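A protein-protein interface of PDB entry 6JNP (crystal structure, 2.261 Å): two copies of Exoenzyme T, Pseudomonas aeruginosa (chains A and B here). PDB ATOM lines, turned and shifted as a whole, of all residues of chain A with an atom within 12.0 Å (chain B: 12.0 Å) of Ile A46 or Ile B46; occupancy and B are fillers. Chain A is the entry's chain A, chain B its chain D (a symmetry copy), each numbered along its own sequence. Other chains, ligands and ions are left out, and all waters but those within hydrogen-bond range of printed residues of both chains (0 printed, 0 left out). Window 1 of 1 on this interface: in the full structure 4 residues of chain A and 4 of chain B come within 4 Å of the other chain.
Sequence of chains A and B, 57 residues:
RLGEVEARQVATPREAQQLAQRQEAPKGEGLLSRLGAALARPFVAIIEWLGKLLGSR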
ATOM      1  N   LEU A  39      31.376  11.716  -3.639  1.00  0.00           N
ATOM      2  CA  LEU A  39      30.410  12.757  -3.326  1.00  0.00           C
ATOM      3  C   LEU A  39      29.415  12.886  -4.469  1.00  0.00           C
ATOM      4  O   LEU A  39      29.799  12.933  -5.642  1.00  0.00           O
ATOM      5  CB  LEU A  39      31.112  14.090  -3.077  1.00  0.00           C
ATOM      6  CG  LEU A  39      30.186  15.237  -2.667  1.00  0.00           C
ATOM      7  CD1 LEU A  39      29.569  14.975  -1.297  1.00  0.00           C
ATOM      8  CD2 LEU A  39      30.920  16.569  -2.685  1.00  0.00           C
ATOM      9  N   ALA A  40      28.135  12.937  -4.126  1.00  0.00           N
ATOM     10  CA  ALA A  40      27.067  13.014  -5.108  1.00  0.00           C
ATOM     11  C   ALA A  40      26.481  14.417  -5.131  1.00  0.00           C
ATOM     12  O   ALA A  40      26.379  15.078  -4.091  1.00  0.00           O
ATOM     13  CB  ALA A  40      25.969  11.993  -4.803  1.00  0.00           C
ATOM     14  N   ARG A  41      26.107  14.872  -6.327  1.00  0.00           N
ATOM     15  CA  ARG A  41      25.407  16.137  -6.531  1.00  0.00           C
ATOM     16  C   ARG A  41      24.070  15.804  -7.181  1.00  0.00           C
ATOM     17  O   ARG A  41      23.885  16.008  -8.391  1.00  0.00           O
ATOM     18  CB  ARG A  41      26.231  17.098  -7.387  1.00  0.00           C
ATOM     19  CG  ARG A  41      27.564  17.486  -6.768  1.00  0.00           C
ATOM     20  CD  ARG A  41      28.401  18.317  -7.728  1.00  0.00           C
ATOM     21  NE  ARG A  41      28.851  17.539  -8.878  1.00  0.00           N
ATOM     22  CZ  ARG A  41      29.593  18.027  -9.866  1.00  0.00           C
ATOM     23  NH1 ARG A  41      29.973  19.297  -9.847  1.00  0.00           N
ATOM     24  NH2 ARG A  41      29.958  17.244 -10.874  1.00  0.00           N
ATOM     25  N   PRO A  42      23.112  15.285  -6.407  1.00  0.00           N
ATOM     26  CA  PRO A  42      21.880  14.753  -7.009  1.00  0.00           C
ATOM     27  C   PRO A  42      20.965  15.825  -7.577  1.00  0.00           C
ATOM     28  O   PRO A  42      21.294  17.016  -7.558  1.00  0.00           O
ATOM     29  CB  PRO A  42      21.215  14.013  -5.842  1.00  0.00           C
ATOM     30  CG  PRO A  42      21.721  14.701  -4.625  1.00  0.00           C
ATOM     31  CD  PRO A  42      23.125  15.135  -4.941  1.00  0.00           C
ATOM     32  N   PHE A  43      19.814  15.390  -8.094  1.00  0.00           N
ATOM     33  CA  PHE A  43      18.833  16.301  -8.671  1.00  0.00           C
ATOM     34  C   PHE A  43      18.472  17.408  -7.691  1.00  0.00           C
ATOM     35  O   PHE A  43      18.407  17.188  -6.478  1.00  0.00           O
ATOM     36  CB  PHE A  43      17.561  15.536  -9.055  1.00  0.00           C
ATOM     37  CG  PHE A  43      17.659  14.781 -10.350  1.00  0.00           C
ATOM     38  CD1 PHE A  43      18.337  13.576 -10.418  1.00  0.00           C
ATOM     39  CD2 PHE A  43      17.043  15.262 -11.493  1.00  0.00           C
ATOM     40  CE1 PHE A  43      18.416  12.876 -11.607  1.00  0.00           C
ATOM     41  CE2 PHE A  43      17.117  14.566 -12.683  1.00  0.00           C
ATOM     42  CZ  PHE A  43      17.803  13.371 -12.740  1.00  0.00           C
ATOM     43  N   VAL A  44      18.237  18.607  -8.230  1.00  0.00           N
ATOM     44  CA  VAL A  44      17.646  19.676  -7.429  1.00  0.00           C
ATOM     45  C   VAL A  44      16.340  19.196  -6.812  1.00  0.00           C
ATOM     46  O   VAL A  44      16.032  19.498  -5.651  1.00  0.00           O
ATOM     47  CB  VAL A  44      17.438  20.939  -8.288  1.00  0.00           C
ATOM     48  CG1 VAL A  44      16.718  22.016  -7.492  1.00  0.00           C
ATOM     49  CG2 VAL A  44      18.772  21.456  -8.810  1.00  0.00           C
ATOM     50  N   ALA A  45      15.562  18.427  -7.577  1.00  0.00           N
ATOM     51  CA  ALA A  45      14.350  17.820  -7.038  1.00  0.00           C
ATOM     52  C   ALA A  45      14.669  16.905  -5.864  1.00  0.00           C
ATOM     53  O   ALA A  45      13.942  16.890  -4.865  1.00  0.00           O
ATOM     54  CB  ALA A  45      13.617  17.051  -8.137  1.00  0.00           C
ATOM     55  N   ILE A  46      15.765  16.148  -5.956  1.00  0.00           N
ATOM     56  CA  ILE A  46      16.145  15.256  -4.863  1.00  0.00           C
ATOM     57  C   ILE A  46      16.598  16.057  -3.648  1.00  0.00           C
ATOM     58  O   ILE A  46      16.310  15.685  -2.507  1.00  0.00           O
ATOM     59  CB  ILE A  46      17.227  14.265  -5.331  1.00  0.00           C
ATOM     60  CG1 ILE A  46      16.625  13.243  -6.296  1.00  0.00           C
ATOM     61  CG2 ILE A  46      17.866  13.561  -4.143  1.00  0.00           C
ATOM     62  CD1 ILE A  46      17.618  12.213  -6.788  1.00  0.00           C
ATOM     63  N   ILE A  47      17.302  17.171  -3.868  1.00  0.00           N
ATOM     64  CA  ILE A  47      17.714  18.025  -2.754  1.00  0.00           C
ATOM     65  C   ILE A  47      16.490  18.588  -2.038  1.00  0.00           C
ATOM     66  O   ILE A  47      16.400  18.565  -0.803  1.00  0.00           O
ATOM     67  CB  ILE A  47      18.637  19.153  -3.251  1.00  0.00           C
ATOM     68  CG1 ILE A  47      19.847  18.580  -3.991  1.00  0.00           C
ATOM     69  CG2 ILE A  47      19.093  20.019  -2.085  1.00  0.00           C
ATOM     70  CD1 ILE A  47      20.812  17.841  -3.100  1.00  0.00           C
ATOM     71  N   GLU A  48      15.533  19.111  -2.809  1.00  0.00           N
ATOM     72  CA  GLU A  48      14.311  19.643  -2.214  1.00  0.00           C
ATOM     73  C   GLU A  48      13.533  18.550  -1.498  1.00  0.00           C
ATOM     74  O   GLU A  48      12.946  18.790  -0.437  1.00  0.00           O
ATOM     75  CB  GLU A  48      13.441  20.301  -3.285  1.00  0.00           C
ATOM     76  CG  GLU A  48      14.111  21.442  -4.033  1.00  0.00           C
ATOM     77  CD  GLU A  48      13.180  22.113  -5.026  1.00  0.00           C
ATOM     78  OE1 GLU A  48      12.880  23.312  -4.847  1.00  0.00           O
ATOM     79  OE2 GLU A  48      12.739  21.438  -5.981  1.00  0.00           O
ATOM     80  N   TRP A  49      13.516  17.341  -2.060  1.00  0.00           N
ATOM     81  CA  TRP A  49      12.816  16.236  -1.419  1.00  0.00           C
ATOM     82  C   TRP A  49      13.493  15.837  -0.115  1.00  0.00           C
ATOM     83  O   TRP A  49      12.816  15.524   0.868  1.00  0.00           O
ATOM     84  CB  TRP A  49      12.732  15.048  -2.375  1.00  0.00           C
ATOM     85  CG  TRP A  49      12.284  13.782  -1.722  1.00  0.00           C
ATOM     86  CD1 TRP A  49      10.999  13.371  -1.523  1.00  0.00           C
ATOM     87  CD2 TRP A  49      13.123  12.755  -1.180  1.00  0.00           C
ATOM     88  NE1 TRP A  49      10.986  12.152  -0.890  1.00  0.00           N
ATOM     89  CE2 TRP A  49      12.277  11.752  -0.669  1.00  0.00           C
ATOM     90  CE3 TRP A  49      14.508  12.589  -1.078  1.00  0.00           C
ATOM     91  CZ2 TRP A  49      12.770  10.599  -0.065  1.00  0.00           C
ATOM     92  CZ3 TRP A  49      14.994  11.441  -0.479  1.00  0.00           C
ATOM     93  CH2 TRP A  49      14.127  10.463   0.021  1.00  0.00           C
ATOM     94  N   LEU A  50      14.827  15.851  -0.084  1.00  0.00           N
ATOM     95  CA  LEU A  50      15.552  15.583   1.154  1.00  0.00           C
ATOM     96  C   LEU A  50      15.223  16.628   2.211  1.00  0.00           C
ATOM     97  O   LEU A  50      14.991  16.298   3.380  1.00  0.00           O
ATOM     98  CB  LEU A  50      17.057  15.552   0.883  1.00  0.00           C
ATOM     99  CG  LEU A  50      17.605  14.356   0.109  1.00  0.00           C
ATOM    100  CD1 LEU A  50      18.990  14.656  -0.441  1.00  0.00           C
ATOM    101  CD2 LEU A  50      17.648  13.145   1.013  1.00  0.00           C
ATOM    102  N   GLY A  51      15.206  17.901   1.815  1.00  0.00           N
ATOM    103  CA  GLY A  51      14.864  18.950   2.763  1.00  0.00           C
ATOM    104  C   GLY A  51      13.445  18.821   3.287  1.00  0.00           C
ATOM    105  O   GLY A  51      13.201  18.951   4.490  1.00  0.00           O
ATOM    106  N   LYS A  52      12.493  18.554   2.390  1.00  0.00           N
ATOM    107  CA  LYS A  52      11.100  18.387   2.788  1.00  0.00           C
ATOM    108  C   LYS A  52      10.909  17.154   3.662  1.00  0.00           C
ATOM    109  O   LYS A  52      10.063  17.158   4.563  1.00  0.00           O
ATOM    110  CB  LYS A  52      10.219  18.307   1.540  1.00  0.00           C
ATOM    111  CG  LYS A  52       8.763  17.967   1.802  1.00  0.00           C
ATOM    112  CD  LYS A  52       7.998  17.826   0.497  1.00  0.00           C
ATOM    113  CE  LYS A  52       6.560  17.403   0.743  1.00  0.00           C
ATOM    114  NZ  LYS A  52       5.783  17.300  -0.523  1.00  0.00           N
ATOM    115  N   LEU A  53      11.691  16.102   3.420  1.00  0.00           N
ATOM    116  CA  LEU A  53      11.593  14.891   4.224  1.00  0.00           C
ATOM    117  C   LEU A  53      12.159  15.114   5.620  1.00  0.00           C
ATOM    118  O   LEU A  53      11.529  14.753   6.621  1.00  0.00           O
ATOM    119  CB  LEU A  53      12.322  13.750   3.519  1.00  0.00           C
ATOM    120  CG  LEU A  53      12.569  12.467   4.312  1.00  0.00           C
ATOM    121  CD1 LEU A  53      11.271  11.702   4.538  1.00  0.00           C
ATOM    122  CD2 LEU A  53      13.597  11.611   3.592  1.00  0.00           C
ATOM    123  N   LEU A  54      13.348  15.713   5.709  1.00  0.00           N
ATOM    124  CA  LEU A  54      13.970  15.934   7.008  1.00  0.00           C
ATOM    125  C   LEU A  54      13.270  17.022   7.810  1.00  0.00           C
ATOM    126  O   LEU A  54      13.369  17.026   9.042  1.00  0.00           O
ATOM    127  CB  LEU A  54      15.446  16.282   6.828  1.00  0.00           C
ATOM    128  CG  LEU A  54      16.263  15.186   6.146  1.00  0.00           C
ATOM    129  CD1 LEU A  54      17.704  15.623   5.990  1.00  0.00           C
ATOM    130  CD2 LEU A  54      16.168  13.883   6.927  1.00  0.00           C
ATOM    131  N   GLY A  55      12.571  17.944   7.145  1.00  0.00           N
ATOM    132  CA  GLY A  55      11.815  18.951   7.869  1.00  0.00           C
ATOM    133  C   GLY A  55      10.471  18.460   8.356  1.00  0.00           C
ATOM    134  O   GLY A  55       9.962  18.951   9.368  1.00  0.00           O
ATOM    135  N   SER A  56       9.878  17.490   7.656  1.00  0.00           N
ATOM    136  CA  SER A  56       8.594  16.934   8.057  1.00  0.00           C
ATOM    137  C   SER A  56       8.717  15.892   9.159  1.00  0.00           C
ATOM    138  O   SER A  56       7.694  15.482   9.717  1.00  0.00           O
ATOM    139  CB  SER A  56       7.886  16.310   6.851  1.00  0.00           C
ATOM    140  OG  SER A  56       8.557  15.142   6.407  1.00  0.00           O
ATOM    141  N   LEU B  39      15.534  -0.980 -16.814  1.00  0.00           N
ATOM    142  CA  LEU B  39      14.457  -0.034 -16.564  1.00  0.00           C
ATOM    143  C   LEU B  39      14.608   0.543 -15.163  1.00  0.00           C
ATOM    144  O   LEU B  39      14.850  -0.191 -14.200  1.00  0.00           O
ATOM    145  CB  LEU B  39      13.096  -0.710 -16.725  1.00  0.00           C
ATOM    146  CG  LEU B  39      11.876   0.190 -16.961  1.00  0.00           C
ATOM    147  CD1 LEU B  39      10.819  -0.565 -17.753  1.00  0.00           C
ATOM    148  CD2 LEU B  39      11.291   0.701 -15.651  1.00  0.00           C
ATOM    149  N   ALA B  40      14.470   1.858 -15.050  1.00  0.00           N
ATOM    150  CA  ALA B  40      14.642   2.556 -13.786  1.00  0.00           C
ATOM    151  C   ALA B  40      13.312   3.124 -13.317  1.00  0.00           C
ATOM    152  O   ALA B  40      12.506   3.598 -14.125  1.00  0.00           O
ATOM    153  CB  ALA B  40      15.674   3.679 -13.914  1.00  0.00           C
ATOM    154  N   ARG B  41      13.085   3.064 -12.005  1.00  0.00           N
ATOM    155  CA  ARG B  41      11.916   3.653 -11.358  1.00  0.00           C
ATOM    156  C   ARG B  41      12.433   4.739 -10.421  1.00  0.00           C
ATOM    157  O   ARG B  41      12.521   4.534  -9.202  1.00  0.00           O
ATOM    158  CB  ARG B  41      11.101   2.596 -10.616  1.00  0.00           C
ATOM    159  CG  ARG B  41      10.768   1.382 -11.471  1.00  0.00           C
ATOM    160  CD  ARG B  41      11.057   0.082 -10.736  1.00  0.00           C
ATOM    161  NE  ARG B  41       9.887  -0.432 -10.031  1.00  0.00           N
ATOM    162  CZ  ARG B  41       9.898  -1.509  -9.252  1.00  0.00           C
ATOM    163  NH1 ARG B  41      11.025  -2.184  -9.069  1.00  0.00           N
ATOM    164  NH2 ARG B  41       8.785  -1.909  -8.651  1.00  0.00           N
ATOM    165  N   PRO B  42      12.788   5.909 -10.959  1.00  0.00           N
ATOM    166  CA  PRO B  42      13.462   6.926 -10.140  1.00  0.00           C
ATOM    167  C   PRO B  42      12.560   7.555  -9.091  1.00  0.00           C
ATOM    168  O   PRO B  42      11.387   7.187  -8.965  1.00  0.00           O
ATOM    169  CB  PRO B  42      13.916   7.961 -11.177  1.00  0.00           C
ATOM    170  CG  PRO B  42      12.938   7.818 -12.292  1.00  0.00           C
ATOM    171  CD  PRO B  42      12.587   6.358 -12.348  1.00  0.00           C
ATOM    172  N   PHE B  43      13.118   8.501  -8.333  1.00  0.00           N
ATOM    173  CA  PHE B  43      12.367   9.213  -7.308  1.00  0.00           C
ATOM    174  C   PHE B  43      11.062   9.761  -7.869  1.00  0.00           C
ATOM    175  O   PHE B  43      10.995  10.179  -9.028  1.00  0.00           O
ATOM    176  CB  PHE B  43      13.199  10.369  -6.747  1.00  0.00           C
ATOM    177  CG  PHE B  43      14.310   9.943  -5.830  1.00  0.00           C
ATOM    178  CD1 PHE B  43      15.482   9.408  -6.337  1.00  0.00           C
ATOM    179  CD2 PHE B  43      14.191  10.105  -4.461  1.00  0.00           C
ATOM    180  CE1 PHE B  43      16.506   9.026  -5.493  1.00  0.00           C
ATOM    181  CE2 PHE B  43      15.211   9.729  -3.613  1.00  0.00           C
ATOM    182  CZ  PHE B  43      16.371   9.187  -4.130  1.00  0.00           C
ATOM    183  N   VAL B  44      10.020   9.757  -7.035  1.00  0.00           N
ATOM    184  CA  VAL B  44       8.779  10.420  -7.423  1.00  0.00           C
ATOM    185  C   VAL B  44       9.027  11.906  -7.636  1.00  0.00           C
ATOM    186  O   VAL B  44       8.348  12.546  -8.446  1.00  0.00           O
ATOM    187  CB  VAL B  44       7.674  10.165  -6.376  1.00  0.00           C
ATOM    188  CG1 VAL B  44       7.433   8.671  -6.214  1.00  0.00           C
ATOM    189  CG2 VAL B  44       8.029  10.805  -5.040  1.00  0.00           C
ATOM    190  N   ALA B  45      10.010  12.473  -6.932  1.00  0.00           N
ATOM    191  CA  ALA B  45      10.408  13.850  -7.197  1.00  0.00           C
ATOM    192  C   ALA B  45      10.986  13.988  -8.599  1.00  0.00           C
ATOM    193  O   ALA B  45      10.688  14.955  -9.309  1.00  0.00           O
ATOM    194  CB  ALA B  45      11.415  14.319  -6.148  1.00  0.00           C
ATOM    195  N   ILE B  46      11.806  13.020  -9.017  1.00  0.00           N
ATOM    196  CA  ILE B  46      12.358  13.038 -10.369  1.00  0.00           C
ATOM    197  C   ILE B  46      11.243  12.921 -11.400  1.00  0.00           C
ATOM    198  O   ILE B  46      11.241  13.628 -12.413  1.00  0.00           O
ATOM    199  CB  ILE B  46      13.406  11.922 -10.541  1.00  0.00           C
ATOM    200  CG1 ILE B  46      14.641  12.202  -9.680  1.00  0.00           C
ATOM    201  CG2 ILE B  46      13.802  11.777 -12.004  1.00  0.00           C
ATOM    202  CD1 ILE B  46      15.744  11.177  -9.848  1.00  0.00           C
ATOM    203  N   ILE B  47      10.273  12.036 -11.154  1.00  0.00           N
ATOM    204  CA  ILE B  47       9.182  11.843 -12.106  1.00  0.00           C
ATOM    205  C   ILE B  47       8.324  13.100 -12.204  1.00  0.00           C
ATOM    206  O   ILE B  47       7.908  13.501 -13.297  1.00  0.00           O
ATOM    207  CB  ILE B  47       8.348  10.610 -11.711  1.00  0.00           C
ATOM    208  CG1 ILE B  47       9.203   9.343 -11.786  1.00  0.00           C
ATOM    209  CG2 ILE B  47       7.120  10.483 -12.601  1.00  0.00           C
ATOM    210  CD1 ILE B  47       8.463   8.079 -11.406  1.00  0.00           C
ATOM    211  N   GLU B  48       8.053  13.748 -11.068  1.00  0.00           N
ATOM    212  CA  GLU B  48       7.267  14.978 -11.093  1.00  0.00           C
ATOM    213  C   GLU B  48       8.020  16.102 -11.795  1.00  0.00           C
ATOM    214  O   GLU B  48       7.425  16.875 -12.557  1.00  0.00           O
ATOM    215  CB  GLU B  48       6.886  15.383  -9.670  1.00  0.00           C
ATOM    216  CG  GLU B  48       5.866  14.458  -9.024  1.00  0.00           C
ATOM    217  CD  GLU B  48       5.751  14.667  -7.527  1.00  0.00           C
ATOM    218  OE1 GLU B  48       6.737  15.123  -6.911  1.00  0.00           O
ATOM    219  OE2 GLU B  48       4.672  14.376  -6.967  1.00  0.00           O
ATOM    220  N   TRP B  49       9.329  16.211 -11.553  1.00  0.00           N
ATOM    221  CA  TRP B  49      10.126  17.205 -12.260  1.00  0.00           C
ATOM    222  C   TRP B  49      10.136  16.936 -13.760  1.00  0.00           C
ATOM    223  O   TRP B  49      10.068  17.872 -14.566  1.00  0.00           O
ATOM    224  CB  TRP B  49      11.548  17.225 -11.698  1.00  0.00           C
ATOM    225  CG  TRP B  49      12.492  18.089 -12.469  1.00  0.00           C
ATOM    226  CD1 TRP B  49      12.575  19.451 -12.430  1.00  0.00           C
ATOM    227  CD2 TRP B  49      13.497  17.650 -13.390  1.00  0.00           C
ATOM    228  NE1 TRP B  49      13.567  19.887 -13.275  1.00  0.00           N
ATOM    229  CE2 TRP B  49      14.149  18.800 -13.875  1.00  0.00           C
ATOM    230  CE3 TRP B  49      13.907  16.397 -13.852  1.00  0.00           C
ATOM    231  CZ2 TRP B  49      15.188  18.735 -14.800  1.00  0.00           C
ATOM    232  CZ3 TRP B  49      14.940  16.334 -14.770  1.00  0.00           C
ATOM    233  CH2 TRP B  49      15.567  17.495 -15.234  1.00  0.00           C
ATOM    234  N   LEU B  50      10.208  15.662 -14.154  1.00  0.00           N
ATOM    235  CA  LEU B  50      10.134  15.313 -15.569  1.00  0.00           C
ATOM    236  C   LEU B  50       8.789  15.706 -16.162  1.00  0.00           C
ATOM    237  O   LEU B  50       8.721  16.195 -17.294  1.00  0.00           O
ATOM    238  CB  LEU B  50      10.374  13.816 -15.762  1.00  0.00           C
ATOM    239  CG  LEU B  50      11.780  13.287 -15.489  1.00  0.00           C
ATOM    240  CD1 LEU B  50      11.860  11.800 -15.789  1.00  0.00           C
ATOM    241  CD2 LEU B  50      12.797  14.055 -16.302  1.00  0.00           C
ATOM    242  N   GLY B  51       7.705  15.478 -15.418  1.00  0.00           N
ATOM    243  CA  GLY B  51       6.395  15.885 -15.900  1.00  0.00           C
ATOM    244  C   GLY B  51       6.299  17.385 -16.100  1.00  0.00           C
ATOM    245  O   GLY B  51       5.806  17.859 -17.129  1.00  0.00           O
ATOM    246  N   LYS B  52       6.781  18.152 -15.119  1.00  0.00           N
ATOM    247  CA  LYS B  52       6.792  19.608 -15.251  1.00  0.00           C
ATOM    248  C   LYS B  52       7.637  20.048 -16.440  1.00  0.00           C
ATOM    249  O   LYS B  52       7.258  20.967 -17.175  1.00  0.00           O
ATOM    250  CB  LYS B  52       7.317  20.253 -13.968  1.00  0.00           C
ATOM    251  CG  LYS B  52       6.557  19.880 -12.707  1.00  0.00           C
ATOM    252  CD  LYS B  52       7.343  20.281 -11.466  1.00  0.00           C
ATOM    253  CE  LYS B  52       6.763  19.653 -10.209  1.00  0.00           C
ATOM    254  NZ  LYS B  52       7.611  19.920  -9.013  1.00  0.00           N
ATOM    255  N   LEU B  53       8.784  19.399 -16.646  1.00  0.00           N
ATOM    256  CA  LEU B  53       9.695  19.799 -17.713  1.00  0.00           C
ATOM    257  C   LEU B  53       9.122  19.479 -19.088  1.00  0.00           C
ATOM    258  O   LEU B  53       9.227  20.289 -20.015  1.00  0.00           O
ATOM    259  CB  LEU B  53      11.043  19.109 -17.520  1.00  0.00           C
ATOM    260  CG  LEU B  53      12.117  19.349 -18.578  1.00  0.00           C
ATOM    261  CD1 LEU B  53      12.701  20.747 -18.446  1.00  0.00           C
ATOM    262  CD2 LEU B  53      13.195  18.287 -18.464  1.00  0.00           C
ATOM    263  N   LEU B  54       8.517  18.300 -19.242  1.00  0.00           N
ATOM    264  CA  LEU B  54       7.954  17.903 -20.523  1.00  0.00           C
ATOM    265  C   LEU B  54       6.601  18.546 -20.795  1.00  0.00           C
ATOM    266  O   LEU B  54       6.147  18.537 -21.943  1.00  0.00           O
ATOM    267  CB  LEU B  54       7.826  16.380 -20.591  1.00  0.00           C
ATOM    268  CG  LEU B  54       9.144  15.610 -20.466  1.00  0.00           C
ATOM    269  CD1 LEU B  54       8.887  14.119 -20.331  1.00  0.00           C
ATOM    270  CD2 LEU B  54      10.053  15.897 -21.653  1.00  0.00           C
ATOM    271  N   GLY B  55       5.950  19.097 -19.773  1.00  0.00           N
ATOM    272  CA  GLY B  55       4.705  19.809 -19.980  1.00  0.00           C
ATOM    273  C   GLY B  55       4.909  21.284 -20.252  1.00  0.00           C
ATOM    274  O   GLY B  55       4.159  21.890 -21.025  1.00  0.00           O
ATOM    275  N   SER B  56       5.926  21.875 -19.627  1.00  0.00           N
ATOM    276  CA  SER B  56       6.197  23.301 -19.762  1.00  0.00           C
ATOM    277  C   SER B  56       7.266  23.619 -20.796  1.00  0.00           C
ATOM    278  O   SER B  56       7.171  24.652 -21.468  1.00  0.00           O
ATOM    279  CB  SER B  56       6.622  23.891 -18.412  1.00  0.00           C
ATOM    280  OG  SER B  56       7.805  23.272 -17.934  1.00  0.00           O
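CD1 of Phe A43 touches CD1 of Ile B46 (3.6 Å). CE2 of Phe A43 touches CZ3 of Trp B49 (3.5 Å). Ala A45 touches Ala B45. CD1 of Ile A46 touches CD1 of Phe B43, at 3.6 Å. CD1 of Ile B46 touches CD1 of Ile A46, 3.7 Å away. Trp A49 touches Phe B43.
Of chain B, only Phe B43 (3.6 Å) and Ile B46 (3.7 Å) come within 4 Å of Ile A46. Ile B46 touches just these residues of chain A: Phe A43 (3.6 Å) and Ile A46 (3.7 Å). Of the printed residues of chain B, Phe A43 touches Ile B46 and Trp B49. Printed residues of chain B within 4 Å of Ala A45: Ala B45. No residue of chain B comes within 4 Å of Glu A48. Trp A49 touches just one residue of chain B: Phe B43 (3.6 Å). No residue of chain B comes within 4 Å of Leu A50. Phe B43 touches just these residues of chain A: Ile A46 and Trp A49. No residue of chain A comes within 4 Å of Val B44. Ala B45 touches one residue of chain A. No residue of chain A comes within 4 Å of Glu B48. Of the printed residues of chain A, Trp B49 touches Phe A43. No residue of chain A comes within 4 Å of Leu B50. The nearest residue of chain B that does not touch Ile A46 is Ala B45 (4.7 Å).
Of the 18 printed residues of chain A, 4 touch a printed residue of chain B. Printed residues of chain A that touch a printed residue of chain B: Phe A43, Ala A45, Ile A46 and Trp A49. Hydrophobic or aromatic side chains of chain A that line the printed part of chain B: Phe A43, Ala A45, Ile A46 and Trp A49. Of the 18 printed residues of chain B, 4 touch a printed residue of chain A. Printed residues of chain B that touch a printed residue of chain A: Phe B43, Ala B45, Ile B46 and Trp B49. Hydrophobic or aromatic side chains of chain B that line the printed part of chain A: Phe B43, Ala B45, Ile B46 and Trp B49. Among the printed residues, 6 pairs touch across the chains. Among the printed residues, no Asp or Glu carboxylate lies within 4 Å of a Lys or Arg side-chain nitrogen of the other chain.
Phe A43 touches Ile B46, and with the chains exchanged Ile A46 touches Phe B43. Phe A43 touches Trp B49, and with the chains exchanged Trp A49 touches Phe B43. Ala A45 touches its own counterpart, Ala B45. Ile B46 touches its own counterpart, Ile A46. Of the 6 pairs that touch across the chains among the printed residues, 6 have their exchanged pair printed and touching as well.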
